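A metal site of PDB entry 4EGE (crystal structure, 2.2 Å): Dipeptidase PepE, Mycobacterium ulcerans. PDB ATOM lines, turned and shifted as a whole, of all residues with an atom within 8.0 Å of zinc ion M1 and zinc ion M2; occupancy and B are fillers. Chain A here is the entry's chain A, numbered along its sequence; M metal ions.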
ATOM      1  N   PHE A 204      17.565 -16.531  10.484  1.00  0.00           N
ATOM      2  CA  PHE A 204      18.106 -15.522   9.589  1.00  0.00           C
ATOM      3  C   PHE A 204      19.562 -15.306   9.941  1.00  0.00           C
ATOM      4  O   PHE A 204      19.958 -15.474  11.109  1.00  0.00           O
ATOM      5  CB  PHE A 204      17.352 -14.188   9.746  1.00  0.00           C
ATOM      6  CG  PHE A 204      17.346 -13.675  11.172  1.00  0.00           C
ATOM      7  CD1 PHE A 204      18.385 -12.847  11.630  1.00  0.00           C
ATOM      8  CD2 PHE A 204      16.332 -14.036  12.053  1.00  0.00           C
ATOM      9  CE1 PHE A 204      18.392 -12.376  12.936  1.00  0.00           C
ATOM     10  CE2 PHE A 204      16.338 -13.580  13.362  1.00  0.00           C
ATOM     11  CZ  PHE A 204      17.374 -12.754  13.803  1.00  0.00           C
ATOM     12  N   ILE A 206      22.482 -12.325   9.026  1.00  0.00           N
ATOM     13  CA  ILE A 206      22.865 -11.067   8.398  1.00  0.00           C
ATOM     14  C   ILE A 206      24.346 -10.848   8.697  1.00  0.00           C
ATOM     15  O   ILE A 206      24.747 -10.882   9.850  1.00  0.00           O
ATOM     16  CB  ILE A 206      21.988  -9.889   8.915  1.00  0.00           C
ATOM     17  CG1 ILE A 206      20.499 -10.060   8.515  1.00  0.00           C
ATOM     18  CG2 ILE A 206      22.540  -8.543   8.419  1.00  0.00           C
ATOM     19  CD1 ILE A 206      19.548  -9.274   9.409  1.00  0.00           C
ATOM     20  N   VAL A 233      26.704  -8.282  12.577  1.00  0.00           N
ATOM     21  CA  VAL A 233      26.271  -9.692  12.555  1.00  0.00           C
ATOM     22  C   VAL A 233      24.989  -9.862  13.393  1.00  0.00           C
ATOM     23  O   VAL A 233      25.010  -9.720  14.627  1.00  0.00           O
ATOM     24  CB  VAL A 233      27.375 -10.687  12.995  1.00  0.00           C
ATOM     25  CG1 VAL A 233      26.883 -12.128  12.935  1.00  0.00           C
ATOM     26  CG2 VAL A 233      28.628 -10.542  12.125  1.00  0.00           C
ATOM     27  N   ASP A 234      23.899 -10.132  12.683  1.00  0.00           N
ATOM     28  CA  ASP A 234      22.556 -10.185  13.247  1.00  0.00           C
ATOM     29  C   ASP A 234      22.015 -11.549  12.888  1.00  0.00           C
ATOM     30  O   ASP A 234      21.835 -11.850  11.714  1.00  0.00           O
ATOM     31  CB  ASP A 234      21.679  -9.091  12.625  1.00  0.00           C
ATOM     32  CG  ASP A 234      20.366  -8.889  13.360  1.00  0.00           C
ATOM     33  OD1 ASP A 234      20.000  -9.753  14.205  1.00  0.00           O
ATOM     34  OD2 ASP A 234      19.719  -7.834  13.122  1.00  0.00           O
ATOM     35  N   ILE A 235      21.752 -12.373  13.893  1.00  0.00           N
ATOM     36  CA  ILE A 235      21.510 -13.781  13.651  1.00  0.00           C
ATOM     37  C   ILE A 235      20.486 -14.295  14.651  1.00  0.00           C
ATOM     38  O   ILE A 235      20.375 -13.776  15.806  1.00  0.00           O
ATOM     39  CB  ILE A 235      22.835 -14.606  13.732  1.00  0.00           C
ATOM     40  CG1 ILE A 235      23.564 -14.355  15.053  1.00  0.00           C
ATOM     41  CG2 ILE A 235      23.768 -14.274  12.550  1.00  0.00           C
ATOM     42  CD1 ILE A 235      24.685 -15.323  15.361  1.00  0.00           C
ATOM     43  N   GLY A 236      19.733 -15.311  14.221  1.00  0.00           N
ATOM     44  CA  GLY A 236      18.804 -15.985  15.115  1.00  0.00           C
ATOM     45  C   GLY A 236      18.420 -17.355  14.609  1.00  0.00           C
ATOM     46  O   GLY A 236      18.631 -17.691  13.426  1.00  0.00           O
ATOM     47  N   SER A 245      15.563 -16.734  18.892  1.00  0.00           N
ATOM     48  CA  SER A 245      16.699 -15.936  19.330  1.00  0.00           C
ATOM     49  C   SER A 245      16.893 -14.846  18.257  1.00  0.00           C
ATOM     50  O   SER A 245      16.398 -14.983  17.118  1.00  0.00           O
ATOM     51  CB  SER A 245      17.932 -16.814  19.490  1.00  0.00           C
ATOM     52  OG  SER A 245      18.296 -17.390  18.219  1.00  0.00           O
ATOM     53  N   ASP A 246      17.561 -13.747  18.631  1.00  0.00           N
ATOM     54  CA  ASP A 246      17.767 -12.602  17.768  1.00  0.00           C
ATOM     55  C   ASP A 246      18.740 -11.673  18.460  1.00  0.00           C
ATOM     56  O   ASP A 246      18.346 -10.885  19.343  1.00  0.00           O
ATOM     57  CB  ASP A 246      16.442 -11.876  17.476  1.00  0.00           C
ATOM     58  CG  ASP A 246      16.598 -10.683  16.531  1.00  0.00           C
ATOM     59  OD1 ASP A 246      17.665 -10.556  15.871  1.00  0.00           O
ATOM     60  OD2 ASP A 246      15.651  -9.864  16.445  1.00  0.00           O
ATOM     61  N   SER A 247      20.006 -11.774  18.064  1.00  0.00           N
ATOM     62  CA  SER A 247      21.062 -10.948  18.650  1.00  0.00           C
ATOM     63  C   SER A 247      22.082 -10.379  17.636  1.00  0.00           C
ATOM     64  O   SER A 247      22.589 -11.094  16.768  1.00  0.00           O
ATOM     65  CB  SER A 247      21.777 -11.747  19.733  1.00  0.00           C
ATOM     66  OG  SER A 247      22.625 -10.915  20.482  1.00  0.00           O
ATOM     67  N   THR A 248      22.409  -9.094  17.768  1.00  0.00           N
ATOM     68  CA  THR A 248      23.384  -8.453  16.870  1.00  0.00           C
ATOM     69  C   THR A 248      24.580  -8.023  17.684  1.00  0.00           C
ATOM     70  O   THR A 248      24.424  -7.462  18.770  1.00  0.00           O
ATOM     71  CB  THR A 248      22.800  -7.207  16.164  1.00  0.00           C
ATOM     72  OG1 THR A 248      21.543  -7.518  15.575  1.00  0.00           O
ATOM     73  CG2 THR A 248      23.716  -6.691  15.088  1.00  0.00           C
ATOM     74  N   ARG A 249      25.782  -8.258  17.142  1.00  0.00           N
ATOM     75  CA  ARG A 249      27.001  -7.714  17.692  1.00  0.00           C
ATOM     76  C   ARG A 249      27.804  -7.212  16.527  1.00  0.00           C
ATOM     77  O   ARG A 249      27.665  -7.747  15.433  1.00  0.00           O
ATOM     78  CB  ARG A 249      27.789  -8.768  18.479  1.00  0.00           C
ATOM     79  CG  ARG A 249      27.188  -9.129  19.846  1.00  0.00           C
ATOM     80  CD  ARG A 249      27.108  -7.912  20.759  1.00  0.00           C
ATOM     81  NE  ARG A 249      26.723  -8.264  22.138  1.00  0.00           N
ATOM     82  CZ  ARG A 249      25.465  -8.352  22.567  1.00  0.00           C
ATOM     83  NH1 ARG A 249      24.436  -8.161  21.717  1.00  0.00           N
ATOM     84  NH2 ARG A 249      25.232  -8.650  23.855  1.00  0.00           N
ATOM     85  N   ARG A 307      13.212   2.082  14.825  1.00  0.00           N
ATOM     86  CA  ARG A 307      12.781   1.852  16.182  1.00  0.00           C
ATOM     87  C   ARG A 307      13.851   1.118  17.023  1.00  0.00           C
ATOM     88  O   ARG A 307      14.756   0.473  16.485  1.00  0.00           O
ATOM     89  CB  ARG A 307      11.507   0.995  16.159  1.00  0.00           C
ATOM     90  CG  ARG A 307      11.741  -0.404  15.606  1.00  0.00           C
ATOM     91  CD  ARG A 307      10.447  -1.154  15.386  1.00  0.00           C
ATOM     92  NE  ARG A 307      10.724  -2.498  14.882  1.00  0.00           N
ATOM     93  CZ  ARG A 307       9.882  -3.239  14.166  1.00  0.00           C
ATOM     94  NH1 ARG A 307       8.671  -2.794  13.871  1.00  0.00           N
ATOM     95  NH2 ARG A 307      10.270  -4.460  13.753  1.00  0.00           N
ATOM     96  N   THR A 308      13.722   1.234  18.342  1.00  0.00           N
ATOM     97  CA  THR A 308      14.684   0.658  19.268  1.00  0.00           C
ATOM     98  C   THR A 308      14.520  -0.856  19.383  1.00  0.00           C
ATOM     99  O   THR A 308      15.493  -1.562  19.650  1.00  0.00           O
ATOM    100  CB  THR A 308      14.600   1.333  20.650  1.00  0.00           C
ATOM    101  OG1 THR A 308      15.119   2.650  20.533  1.00  0.00           O
ATOM    102  CG2 THR A 308      15.444   0.573  21.715  1.00  0.00           C
ATOM    103  N   GLY A 309      13.309  -1.367  19.172  1.00  0.00           N
ATOM    104  CA  GLY A 309      13.095  -2.818  19.299  1.00  0.00           C
ATOM    105  C   GLY A 309      11.708  -3.344  18.968  1.00  0.00           C
ATOM    106  O   GLY A 309      10.776  -2.564  18.778  1.00  0.00           O
ATOM    107  N   HIS A 310      11.587  -4.668  18.940  1.00  0.00           N
ATOM    108  CA  HIS A 310      10.339  -5.328  18.597  1.00  0.00           C
ATOM    109  C   HIS A 310      10.114  -6.472  19.547  1.00  0.00           C
ATOM    110  O   HIS A 310      11.064  -7.022  20.098  1.00  0.00           O
ATOM    111  CB  HIS A 310      10.433  -5.875  17.171  1.00  0.00           C
ATOM    112  CG  HIS A 310      11.608  -6.805  16.982  1.00  0.00           C
ATOM    113  ND1 HIS A 310      11.644  -8.035  17.515  1.00  0.00           N
ATOM    114  CD2 HIS A 310      12.844  -6.593  16.384  1.00  0.00           C
ATOM    115  CE1 HIS A 310      12.841  -8.606  17.250  1.00  0.00           C
ATOM    116  NE2 HIS A 310      13.567  -7.728  16.554  1.00  0.00           N
ATOM    117  N   GLY A 311       8.861  -6.847  19.757  1.00  0.00           N
ATOM    118  CA  GLY A 311       8.562  -8.017  20.559  1.00  0.00           C
ATOM    119  C   GLY A 311       9.064  -9.264  19.855  1.00  0.00           C
ATOM    120  O   GLY A 311       9.318  -9.278  18.645  1.00  0.00           O
ATOM    121  N   ILE A 312       9.226 -10.330  20.614  1.00  0.00           N
ATOM    122  CA  ILE A 312       9.691 -11.569  20.034  1.00  0.00           C
ATOM    123  C   ILE A 312       9.010 -12.678  20.828  1.00  0.00           C
ATOM    124  O   ILE A 312       8.668 -12.488  21.986  1.00  0.00           O
ATOM    125  CB  ILE A 312      11.254 -11.643  20.065  1.00  0.00           C
ATOM    126  CG1 ILE A 312      11.785 -12.867  19.299  1.00  0.00           C
ATOM    127  CG2 ILE A 312      11.806 -11.508  21.485  1.00  0.00           C
ATOM    128  CD1 ILE A 312      13.267 -12.756  18.979  1.00  0.00           C
ATOM    129  N   VAL A 316       9.678 -13.716  15.043  1.00  0.00           N
ATOM    130  CA  VAL A 316      10.836 -12.829  15.292  1.00  0.00           C
ATOM    131  C   VAL A 316      10.332 -11.406  15.619  1.00  0.00           C
ATOM    132  O   VAL A 316      10.948 -10.697  16.394  1.00  0.00           O
ATOM    133  CB  VAL A 316      11.835 -12.774  14.115  1.00  0.00           C
ATOM    134  CG1 VAL A 316      13.132 -12.101  14.517  1.00  0.00           C
ATOM    135  CG2 VAL A 316      12.188 -14.161  13.638  1.00  0.00           C
ATOM    136  N   HIS A 317       9.199 -11.013  15.038  1.00  0.00           N
ATOM    137  CA  HIS A 317       8.654  -9.661  15.170  1.00  0.00           C
ATOM    138  C   HIS A 317       7.239  -9.708  15.652  1.00  0.00           C
ATOM    139  O   HIS A 317       6.368 -10.208  14.947  1.00  0.00           O
ATOM    140  CB  HIS A 317       8.708  -8.946  13.811  1.00  0.00           C
ATOM    141  CG  HIS A 317      10.092  -8.474  13.414  1.00  0.00           C
ATOM    142  ND1 HIS A 317      10.316  -7.776  12.281  1.00  0.00           N
ATOM    143  CD2 HIS A 317      11.315  -8.597  14.057  1.00  0.00           C
ATOM    144  CE1 HIS A 317      11.622  -7.463  12.196  1.00  0.00           C
ATOM    145  NE2 HIS A 317      12.247  -7.984  13.278  1.00  0.00           N
ATOM    146  N   PHE A 336      11.145  -8.429  24.237  1.00  0.00           N
ATOM    147  CA  PHE A 336      11.404  -7.627  23.052  1.00  0.00           C
ATOM    148  C   PHE A 336      12.907  -7.389  22.947  1.00  0.00           C
ATOM    149  O   PHE A 336      13.662  -7.600  23.911  1.00  0.00           O
ATOM    150  CB  PHE A 336      10.641  -6.283  23.132  1.00  0.00           C
ATOM    151  CG  PHE A 336      10.741  -5.598  24.471  1.00  0.00           C
ATOM    152  CD1 PHE A 336      11.855  -4.819  24.791  1.00  0.00           C
ATOM    153  CD2 PHE A 336       9.738  -5.755  25.420  1.00  0.00           C
ATOM    154  CE1 PHE A 336      11.955  -4.182  26.013  1.00  0.00           C
ATOM    155  CE2 PHE A 336       9.826  -5.149  26.667  1.00  0.00           C
ATOM    156  CZ  PHE A 336      10.942  -4.353  26.961  1.00  0.00           C
ATOM    157  N   SER A 337      13.319  -6.948  21.769  1.00  0.00           N
ATOM    158  CA  SER A 337      14.687  -6.576  21.503  1.00  0.00           C
ATOM    159  C   SER A 337      14.952  -5.131  21.931  1.00  0.00           C
ATOM    160  O   SER A 337      14.043  -4.322  21.976  1.00  0.00           O
ATOM    161  CB  SER A 337      14.978  -6.714  20.026  1.00  0.00           C
ATOM    162  OG  SER A 337      14.311  -5.694  19.310  1.00  0.00           O
ATOM    163  N   ILE A 338      16.204  -4.850  22.294  1.00  0.00           N
ATOM    164  CA  ILE A 338      16.705  -3.502  22.408  1.00  0.00           C
ATOM    165  C   ILE A 338      17.876  -3.483  21.429  1.00  0.00           C
ATOM    166  O   ILE A 338      18.870  -4.190  21.651  1.00  0.00           O
ATOM    167  CB  ILE A 338      17.161  -3.171  23.840  1.00  0.00           C
ATOM    168  CG1 ILE A 338      15.977  -3.231  24.821  1.00  0.00           C
ATOM    169  CG2 ILE A 338      17.841  -1.804  23.875  1.00  0.00           C
ATOM    170  CD1 ILE A 338      14.908  -2.175  24.591  1.00  0.00           C
ATOM    171  N   GLU A 339      17.769  -2.686  20.368  1.00  0.00           N
ATOM    172  CA  GLU A 339      18.701  -2.768  19.242  1.00  0.00           C
ATOM    173  C   GLU A 339      18.925  -1.453  18.504  1.00  0.00           C
ATOM    174  O   GLU A 339      18.712  -1.365  17.278  1.00  0.00           O
ATOM    175  CB  GLU A 339      18.280  -3.903  18.269  1.00  0.00           C
ATOM    176  CG  GLU A 339      16.830  -3.847  17.780  1.00  0.00           C
ATOM    177  CD  GLU A 339      16.587  -4.807  16.633  1.00  0.00           C
ATOM    178  OE1 GLU A 339      17.323  -4.714  15.619  1.00  0.00           O
ATOM    179  OE2 GLU A 339      15.689  -5.688  16.750  1.00  0.00           O
ATOM    180  N   ARG A 351      25.228  -2.012  15.183  1.00  0.00           N
ATOM    181  CA  ARG A 351      24.008  -2.254  15.913  1.00  0.00           C
ATOM    182  C   ARG A 351      24.327  -3.183  17.090  1.00  0.00           C
ATOM    183  O   ARG A 351      25.125  -4.104  16.977  1.00  0.00           O
ATOM    184  CB  ARG A 351      22.926  -2.881  14.999  1.00  0.00           C
ATOM    185  CG  ARG A 351      21.562  -3.014  15.681  1.00  0.00           C
ATOM    186  CD  ARG A 351      20.420  -3.288  14.702  1.00  0.00           C
ATOM    187  NE  ARG A 351      20.553  -4.535  13.937  1.00  0.00           N
ATOM    188  CZ  ARG A 351      20.963  -4.603  12.676  1.00  0.00           C
ATOM    189  NH1 ARG A 351      21.285  -3.491  12.015  1.00  0.00           N
ATOM    190  NH2 ARG A 351      21.046  -5.778  12.065  1.00  0.00           N
ATOM    191  N   GLU A 353      22.325  -5.539  19.769  1.00  0.00           N
ATOM    192  CA  GLU A 353      20.978  -6.049  19.993  1.00  0.00           C
ATOM    193  C   GLU A 353      20.897  -7.170  21.013  1.00  0.00           C
ATOM    194  O   GLU A 353      21.526  -8.222  20.815  1.00  0.00           O
ATOM    195  CB  GLU A 353      20.343  -6.512  18.686  1.00  0.00           C
ATOM    196  CG  GLU A 353      19.091  -7.346  18.946  1.00  0.00           C
ATOM    197  CD  GLU A 353      18.322  -7.698  17.689  1.00  0.00           C
ATOM    198  OE1 GLU A 353      18.966  -7.889  16.616  1.00  0.00           O
ATOM    199  OE2 GLU A 353      17.078  -7.767  17.803  1.00  0.00           O
ATOM    200  N   ASP A 354      20.110  -6.945  22.061  1.00  0.00           N
ATOM    201  CA  ASP A 354      19.781  -7.980  23.020  1.00  0.00           C
ATOM    202  C   ASP A 354      18.280  -8.180  23.048  1.00  0.00           C
ATOM    203  O   ASP A 354      17.512  -7.225  22.813  1.00  0.00           O
ATOM    204  CB  ASP A 354      20.194  -7.585  24.427  1.00  0.00           C
ATOM    205  CG  ASP A 354      21.679  -7.480  24.600  1.00  0.00           C
ATOM    206  OD1 ASP A 354      22.395  -8.239  23.902  1.00  0.00           O
ATOM    207  OD2 ASP A 354      22.123  -6.625  25.410  1.00  0.00           O
ATOM    208  N   ILE A 355      17.862  -9.421  23.325  1.00  0.00           N
ATOM    209  CA  ILE A 355      16.498  -9.696  23.748  1.00  0.00           C
ATOM    210  C   ILE A 355      16.445  -9.618  25.261  1.00  0.00           C
ATOM    211  O   ILE A 355      17.264 -10.259  25.951  1.00  0.00           O
ATOM    212  CB  ILE A 355      16.017 -11.116  23.333  1.00  0.00           C
ATOM    213  CG1 ILE A 355      16.034 -11.294  21.807  1.00  0.00           C
ATOM    214  CG2 ILE A 355      14.662 -11.428  23.974  1.00  0.00           C
ATOM    215  CD1 ILE A 355      15.454 -10.107  21.044  1.00  0.00           C
HETATM  216 ZN    ZN M   1      18.196  -8.905  14.942  1.00  0.00          ZN
HETATM  217 ZN    ZN M   2      15.641  -7.849  16.246  1.00  0.00          ZN
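Merely in contact with zinc ion M2: Ser 337 (3.98 Å).
Within 4 Å of zinc ion M2: Asp 246, His 310, Ser 337, Glu 339 and Glu 353.
The nearest printed residue that does not touch zinc ion M2 is His 317 (4.5 Å).
Zinc ion M2 is bound by OD2 of Asp 246 (2.0 Å), NE2 of His 310 (2.1 Å), OE2 of Glu 353 (2.1 Å) and OE2 of Glu 339 (2.2 Å).
Zinc ion M2 has four donor atoms within binding distance.
Merely in contact with zinc ion M1: Thr 248 (3.7 Å).
Of the 27 residues printed, 4 come within 4 Å of zinc ion M1.
The guanidinium group (NH1) of Arg 249 is in hydrogen-bond range of the backbone carbonyl oxygen (O) of Glu 353, at 3.0 Å.
The side-chain carboxylate (OE2) of Glu 339 sits close to the side-chain hydroxyl (OG) of Ser 337 (2.9 Å).
The backbone carbonyl oxygen (O) of Glu 353 sits at hydrogen-bond distance from the side-chain hydroxyl (OG) of Ser 247 (2.9 Å).
The guanidinium group of Arg 351 is in salt-bridge range of the side-chain carboxylate of Glu 339 (3.6 Å).
The guanidinium group (NH2) of Arg 351 is in salt-bridge range of the side-chain carboxylate (OD2) of Asp 234 (2.7 Å).
ND1 of His 310 sits close to O of Val 316 (3.0 Å).
The backbone carbonyl oxygen of His 310 sits at hydrogen-bond distance from the backbone NH of Ser 337 (2.8 Å).
The backbone NH (N) of Glu 339 is in hydrogen-bond range of the backbone carbonyl oxygen (O) of Thr 308 (2.6 Å).
Zinc ion M1 is bound by OD1 of Asp 246, 2.0 Å away.
The side-chain carboxylate (OE1) of Glu 353 is bound to zinc ion M1, 2.1 Å away.
OD1 of Asp 234 is bound to zinc ion M1.
Slightly farther from zinc ion M1 lies OD2 of Asp 234 (2.6 Å).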
